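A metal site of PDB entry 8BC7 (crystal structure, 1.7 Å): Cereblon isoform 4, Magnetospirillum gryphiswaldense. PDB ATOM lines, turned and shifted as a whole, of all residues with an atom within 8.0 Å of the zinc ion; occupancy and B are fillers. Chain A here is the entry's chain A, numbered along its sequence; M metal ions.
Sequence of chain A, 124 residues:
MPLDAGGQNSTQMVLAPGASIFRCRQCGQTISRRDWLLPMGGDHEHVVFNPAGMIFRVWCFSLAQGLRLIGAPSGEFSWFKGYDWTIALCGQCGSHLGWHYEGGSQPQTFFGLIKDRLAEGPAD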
ATOM      1  N   ARG A  23     -19.427   4.614 -14.566  1.00  0.00           N
ATOM      2  CA  ARG A  23     -20.036   4.296 -13.257  1.00  0.00           C
ATOM      3  C   ARG A  23     -19.453   5.228 -12.205  1.00  0.00           C
ATOM      4  O   ARG A  23     -18.337   5.720 -12.371  1.00  0.00           O
ATOM      5  CB  ARG A  23     -19.739   2.849 -12.867  1.00  0.00           C
ATOM      6  CG  ARG A  23     -20.443   1.837 -13.753  1.00  0.00           C
ATOM      7  CD  ARG A  23     -20.268   0.382 -13.323  1.00  0.00           C
ATOM      8  NE  ARG A  23     -21.015  -0.506 -14.210  1.00  0.00           N
ATOM      9  CZ  ARG A  23     -22.342  -0.643 -14.205  1.00  0.00           C
ATOM     10  NH1 ARG A  23     -23.060  -0.157 -13.207  1.00  0.00           N
ATOM     11  NH2 ARG A  23     -22.940  -1.380 -15.122  1.00  0.00           N
ATOM     12  N   CYS A  24     -20.179   5.402 -11.100  1.00  0.00           N
ATOM     13  CA  CYS A  24     -19.648   6.101  -9.920  1.00  0.00           C
ATOM     14  C   CYS A  24     -18.406   5.352  -9.431  1.00  0.00           C
ATOM     15  O   CYS A  24     -18.501   4.149  -9.216  1.00  0.00           O
ATOM     16  CB  CYS A  24     -20.715   6.185  -8.839  1.00  0.00           C
ATOM     17  SG  CYS A  24     -20.089   6.926  -7.287  1.00  0.00           S
ATOM     18  N   ARG A  25     -17.261   6.045  -9.291  1.00  0.00           N
ATOM     19  CA  ARG A  25     -15.994   5.414  -8.844  1.00  0.00           C
ATOM     20  C   ARG A  25     -16.134   4.871  -7.412  1.00  0.00           C
ATOM     21  O   ARG A  25     -15.341   3.959  -7.086  1.00  0.00           O
ATOM     22  CB  ARG A  25     -14.894   6.469  -8.952  1.00  0.00           C
ATOM     23  CG  ARG A  25     -13.537   6.073  -8.440  1.00  0.00           C
ATOM     24  CD  ARG A  25     -12.636   7.289  -8.522  1.00  0.00           C
ATOM     25  NE  ARG A  25     -11.374   6.890  -7.956  1.00  0.00           N
ATOM     26  CZ  ARG A  25     -10.290   7.640  -7.949  1.00  0.00           C
ATOM     27  NH1 ARG A  25     -10.252   8.820  -8.593  1.00  0.00           N
ATOM     28  NH2 ARG A  25      -9.250   7.144  -7.356  1.00  0.00           N
ATOM     29  N   GLN A  26     -17.008   5.434  -6.580  1.00  0.00           N
ATOM     30  CA  GLN A  26     -17.129   5.032  -5.144  1.00  0.00           C
ATOM     31  C   GLN A  26     -18.008   3.818  -4.969  1.00  0.00           C
ATOM     32  O   GLN A  26     -17.683   3.004  -4.142  1.00  0.00           O
ATOM     33  CB  GLN A  26     -17.709   6.203  -4.321  1.00  0.00           C
ATOM     34  CG  GLN A  26     -16.786   7.394  -4.336  1.00  0.00           C
ATOM     35  CD  GLN A  26     -15.397   7.040  -3.834  1.00  0.00           C
ATOM     36  OE1 GLN A  26     -15.218   6.223  -2.914  1.00  0.00           O
ATOM     37  NE2 GLN A  26     -14.396   7.636  -4.473  1.00  0.00           N
ATOM     38  N   CYS A  27     -19.049   3.623  -5.773  1.00  0.00           N
ATOM     39  CA  CYS A  27     -20.041   2.557  -5.472  1.00  0.00           C
ATOM     40  C   CYS A  27     -20.407   1.736  -6.720  1.00  0.00           C
ATOM     41  O   CYS A  27     -21.048   0.724  -6.543  1.00  0.00           O
ATOM     42  CB  CYS A  27     -21.227   3.183  -4.788  1.00  0.00           C
ATOM     43  SG  CYS A  27     -22.277   4.083  -5.974  1.00  0.00           S
ATOM     44  N   GLY A  28     -20.136   2.189  -7.942  1.00  0.00           N
ATOM     45  CA  GLY A  28     -20.546   1.397  -9.120  1.00  0.00           C
ATOM     46  C   GLY A  28     -21.883   1.745  -9.761  1.00  0.00           C
ATOM     47  O   GLY A  28     -22.216   1.129 -10.781  1.00  0.00           O
ATOM     48  N   GLN A  29     -22.620   2.699  -9.239  1.00  0.00           N
ATOM     49  CA  GLN A  29     -23.862   3.182  -9.837  1.00  0.00           C
ATOM     50  C   GLN A  29     -23.639   3.475 -11.337  1.00  0.00           C
ATOM     51  O   GLN A  29     -22.698   4.199 -11.627  1.00  0.00           O
ATOM     52  CB  GLN A  29     -24.299   4.439  -9.117  1.00  0.00           C
ATOM     53  CG  GLN A  29     -25.544   5.088  -9.706  1.00  0.00           C
ATOM     54  CD  GLN A  29     -26.809   4.460  -9.194  1.00  0.00           C
ATOM     55  OE1 GLN A  29     -26.950   3.255  -9.120  1.00  0.00           O
ATOM     56  NE2 GLN A  29     -27.785   5.290  -8.842  1.00  0.00           N
ATOM     57  N   THR A  30     -24.522   3.028 -12.199  1.00  0.00           N
ATOM     58  CA  THR A  30     -24.497   3.376 -13.660  1.00  0.00           C
ATOM     59  C   THR A  30     -24.811   4.867 -13.821  1.00  0.00           C
ATOM     60  O   THR A  30     -25.843   5.274 -13.282  1.00  0.00           O
ATOM     61  CB  THR A  30     -25.481   2.526 -14.466  1.00  0.00           C
ATOM     62  OG1 THR A  30     -25.376   1.163 -14.076  1.00  0.00           O
ATOM     63  CG2 THR A  30     -25.125   2.639 -15.919  1.00  0.00           C
ATOM     64  N   ILE A  31     -23.956   5.641 -14.521  1.00  0.00           N
ATOM     65  CA  ILE A  31     -24.126   7.119 -14.612  1.00  0.00           C
ATOM     66  C   ILE A  31     -24.251   7.562 -16.073  1.00  0.00           C
ATOM     67  O   ILE A  31     -25.251   8.238 -16.400  1.00  0.00           O
ATOM     68  CB  ILE A  31     -22.995   7.910 -13.908  1.00  0.00           C
ATOM     69  CG1 ILE A  31     -22.843   7.558 -12.442  1.00  0.00           C
ATOM     70  CG2 ILE A  31     -23.285   9.422 -14.095  1.00  0.00           C
ATOM     71  CD1 ILE A  31     -24.018   7.862 -11.553  1.00  0.00           C
ATOM     72  N   GLY A  66     -28.960   7.793 -12.756  1.00  0.00           N
ATOM     73  CA  GLY A  66     -28.462   7.323 -11.475  1.00  0.00           C
ATOM     74  C   GLY A  66     -27.995   8.453 -10.546  1.00  0.00           C
ATOM     75  O   GLY A  66     -27.326   8.148  -9.551  1.00  0.00           O
ATOM     76  N   LEU A  89     -25.528  14.656  -7.241  1.00  0.00           N
ATOM     77  CA  LEU A  89     -24.919  13.585  -6.414  1.00  0.00           C
ATOM     78  C   LEU A  89     -25.168  12.260  -7.110  1.00  0.00           C
ATOM     79  O   LEU A  89     -26.168  12.105  -7.831  1.00  0.00           O
ATOM     80  CB  LEU A  89     -25.546  13.572  -5.012  1.00  0.00           C
ATOM     81  CG  LEU A  89     -25.449  14.895  -4.230  1.00  0.00           C
ATOM     82  CD1 LEU A  89     -25.973  14.728  -2.797  1.00  0.00           C
ATOM     83  CD2 LEU A  89     -24.048  15.451  -4.238  1.00  0.00           C
ATOM     84  N   CYS A  90     -24.297  11.304  -6.830  1.00  0.00           N
ATOM     85  CA  CYS A  90     -24.609   9.883  -7.086  1.00  0.00           C
ATOM     86  C   CYS A  90     -25.896   9.555  -6.316  1.00  0.00           C
ATOM     87  O   CYS A  90     -25.945   9.782  -5.094  1.00  0.00           O
ATOM     88  CB  CYS A  90     -23.468   8.993  -6.618  1.00  0.00           C
ATOM     89  SG  CYS A  90     -23.820   7.240  -6.903  1.00  0.00           S
ATOM     90  N   GLY A  91     -26.927   9.014  -6.968  1.00  0.00           N
ATOM     91  CA  GLY A  91     -28.195   8.718  -6.309  1.00  0.00           C
ATOM     92  C   GLY A  91     -28.065   7.549  -5.365  1.00  0.00           C
ATOM     93  O   GLY A  91     -28.962   7.302  -4.489  1.00  0.00           O
ATOM     94  N   GLN A  92     -27.020   6.769  -5.506  1.00  0.00           N
ATOM     95  CA  GLN A  92     -26.782   5.583  -4.669  1.00  0.00           C
ATOM     96  C   GLN A  92     -25.990   6.006  -3.406  1.00  0.00           C
ATOM     97  O   GLN A  92     -26.508   5.831  -2.253  1.00  0.00           O
ATOM     98  CB  GLN A  92     -26.161   4.475  -5.485  1.00  0.00           C
ATOM     99  CG  GLN A  92     -26.006   3.186  -4.738  1.00  0.00           C
ATOM    100  CD  GLN A  92     -25.780   2.018  -5.671  1.00  0.00           C
ATOM    101  OE1 GLN A  92     -26.715   1.302  -5.967  1.00  0.00           O
ATOM    102  NE2 GLN A  92     -24.569   1.787  -6.144  1.00  0.00           N
ATOM    103  N   CYS A  93     -24.790   6.540  -3.563  1.00  0.00           N
ATOM    104  CA  CYS A  93     -23.854   6.732  -2.447  1.00  0.00           C
ATOM    105  C   CYS A  93     -23.763   8.190  -2.011  1.00  0.00           C
ATOM    106  O   CYS A  93     -23.215   8.405  -0.929  1.00  0.00           O
ATOM    107  CB  CYS A  93     -22.471   6.157  -2.705  1.00  0.00           C
ATOM    108  SG  CYS A  93     -21.463   7.184  -3.814  1.00  0.00           S
ATOM    109  N   GLY A  94     -24.362   9.125  -2.758  1.00  0.00           N
ATOM    110  CA  GLY A  94     -24.380  10.549  -2.364  1.00  0.00           C
ATOM    111  C   GLY A  94     -23.060  11.282  -2.642  1.00  0.00           C
ATOM    112  O   GLY A  94     -22.921  12.434  -2.245  1.00  0.00           O
ATOM    113  N   SER A  95     -22.092  10.653  -3.287  1.00  0.00           N
ATOM    114  CA  SER A  95     -20.832  11.274  -3.765  1.00  0.00           C
ATOM    115  C   SER A  95     -21.147  12.417  -4.732  1.00  0.00           C
ATOM    116  O   SER A  95     -22.048  12.298  -5.575  1.00  0.00           O
ATOM    117  CB  SER A  95     -19.927  10.213  -4.374  1.00  0.00           C
ATOM    118  OG  SER A  95     -18.811  10.787  -5.072  1.00  0.00           O
ATOM    119  N   HIS A  96     -20.425  13.549  -4.588  1.00  0.00           N
ATOM    120  CA  HIS A  96     -20.621  14.660  -5.545  1.00  0.00           C
ATOM    121  C   HIS A  96     -20.029  14.323  -6.923  1.00  0.00           C
ATOM    122  O   HIS A  96     -18.764  14.179  -6.986  1.00  0.00           O
ATOM    123  CB  HIS A  96     -19.987  15.940  -4.954  1.00  0.00           C
ATOM    124  CG  HIS A  96     -20.177  17.060  -5.888  1.00  0.00           C
ATOM    125  ND1 HIS A  96     -19.227  18.069  -6.038  1.00  0.00           N
ATOM    126  CD2 HIS A  96     -21.151  17.301  -6.820  1.00  0.00           C
ATOM    127  CE1 HIS A  96     -19.675  18.931  -6.917  1.00  0.00           C
ATOM    128  NE2 HIS A  96     -20.851  18.494  -7.419  1.00  0.00           N
ATOM    129  N   LEU A  97     -20.837  14.123  -7.954  1.00  0.00           N
ATOM    130  CA  LEU A  97     -20.321  13.744  -9.263  1.00  0.00           C
ATOM    131  C   LEU A  97     -20.235  14.896 -10.257  1.00  0.00           C
ATOM    132  O   LEU A  97     -19.511  14.759 -11.264  1.00  0.00           O
ATOM    133  CB  LEU A  97     -21.120  12.580  -9.815  1.00  0.00           C
ATOM    134  CG  LEU A  97     -21.034  11.250  -9.063  1.00  0.00           C
ATOM    135  CD1 LEU A  97     -21.775  10.188  -9.832  1.00  0.00           C
ATOM    136  CD2 LEU A  97     -19.601  10.808  -8.797  1.00  0.00           C
ATOM    137  N   ARG A 117     -14.132  11.302 -10.828  1.00  0.00           N
ATOM    138  CA  ARG A 117     -15.138  10.706  -9.925  1.00  0.00           C
ATOM    139  C   ARG A 117     -15.882   9.550 -10.635  1.00  0.00           C
ATOM    140  O   ARG A 117     -16.796   8.988  -9.989  1.00  0.00           O
ATOM    141  CB  ARG A 117     -16.030  11.824  -9.393  1.00  0.00           C
ATOM    142  CG  ARG A 117     -15.161  12.820  -8.647  1.00  0.00           C
ATOM    143  CD  ARG A 117     -15.845  13.683  -7.648  1.00  0.00           C
ATOM    144  NE  ARG A 117     -14.900  14.664  -7.079  1.00  0.00           N
ATOM    145  CZ  ARG A 117     -15.294  15.690  -6.343  1.00  0.00           C
ATOM    146  NH1 ARG A 117     -16.564  15.836  -6.029  1.00  0.00           N
ATOM    147  NH2 ARG A 117     -14.404  16.571  -5.907  1.00  0.00           N
HETATM  148 ZN    ZN M   1     -21.842   6.370  -5.946  1.00  0.00          ZN
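The side-chain sulfur of Cys 27 sits close to the side-chain amide nitrogen of Gln 92, 3.2 Å away. The backbone NH of Gln 26 sits close to the side-chain sulfur of Cys 24. The side-chain sulfur (SG) of Cys 90 sits close to the backbone NH (N) of Gln 92, 3.5 Å away. The backbone NH (N) of Ser 95 lies close to the side-chain sulfur (SG) of Cys 93 (3.6 Å). SG of Cys 27 sits close to N of Gln 29, at 3.6 Å. The backbone carbonyl oxygen of Gln 29 lies within hydrogen-bond range of the backbone NH of Cys 24 (2.8 Å). N of Cys 90 lies within hydrogen-bond range of O of Ser 95 (2.8 Å).
The zinc ion is bound by SG of Cys 24, SG of Cys 93, SG of Cys 27 and SG of Cys 90. The zinc ion has four donor atoms within binding distance.
Within 4 Å of the zinc ion: Cys 24, Cys 27, Cys 90 and Cys 93.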
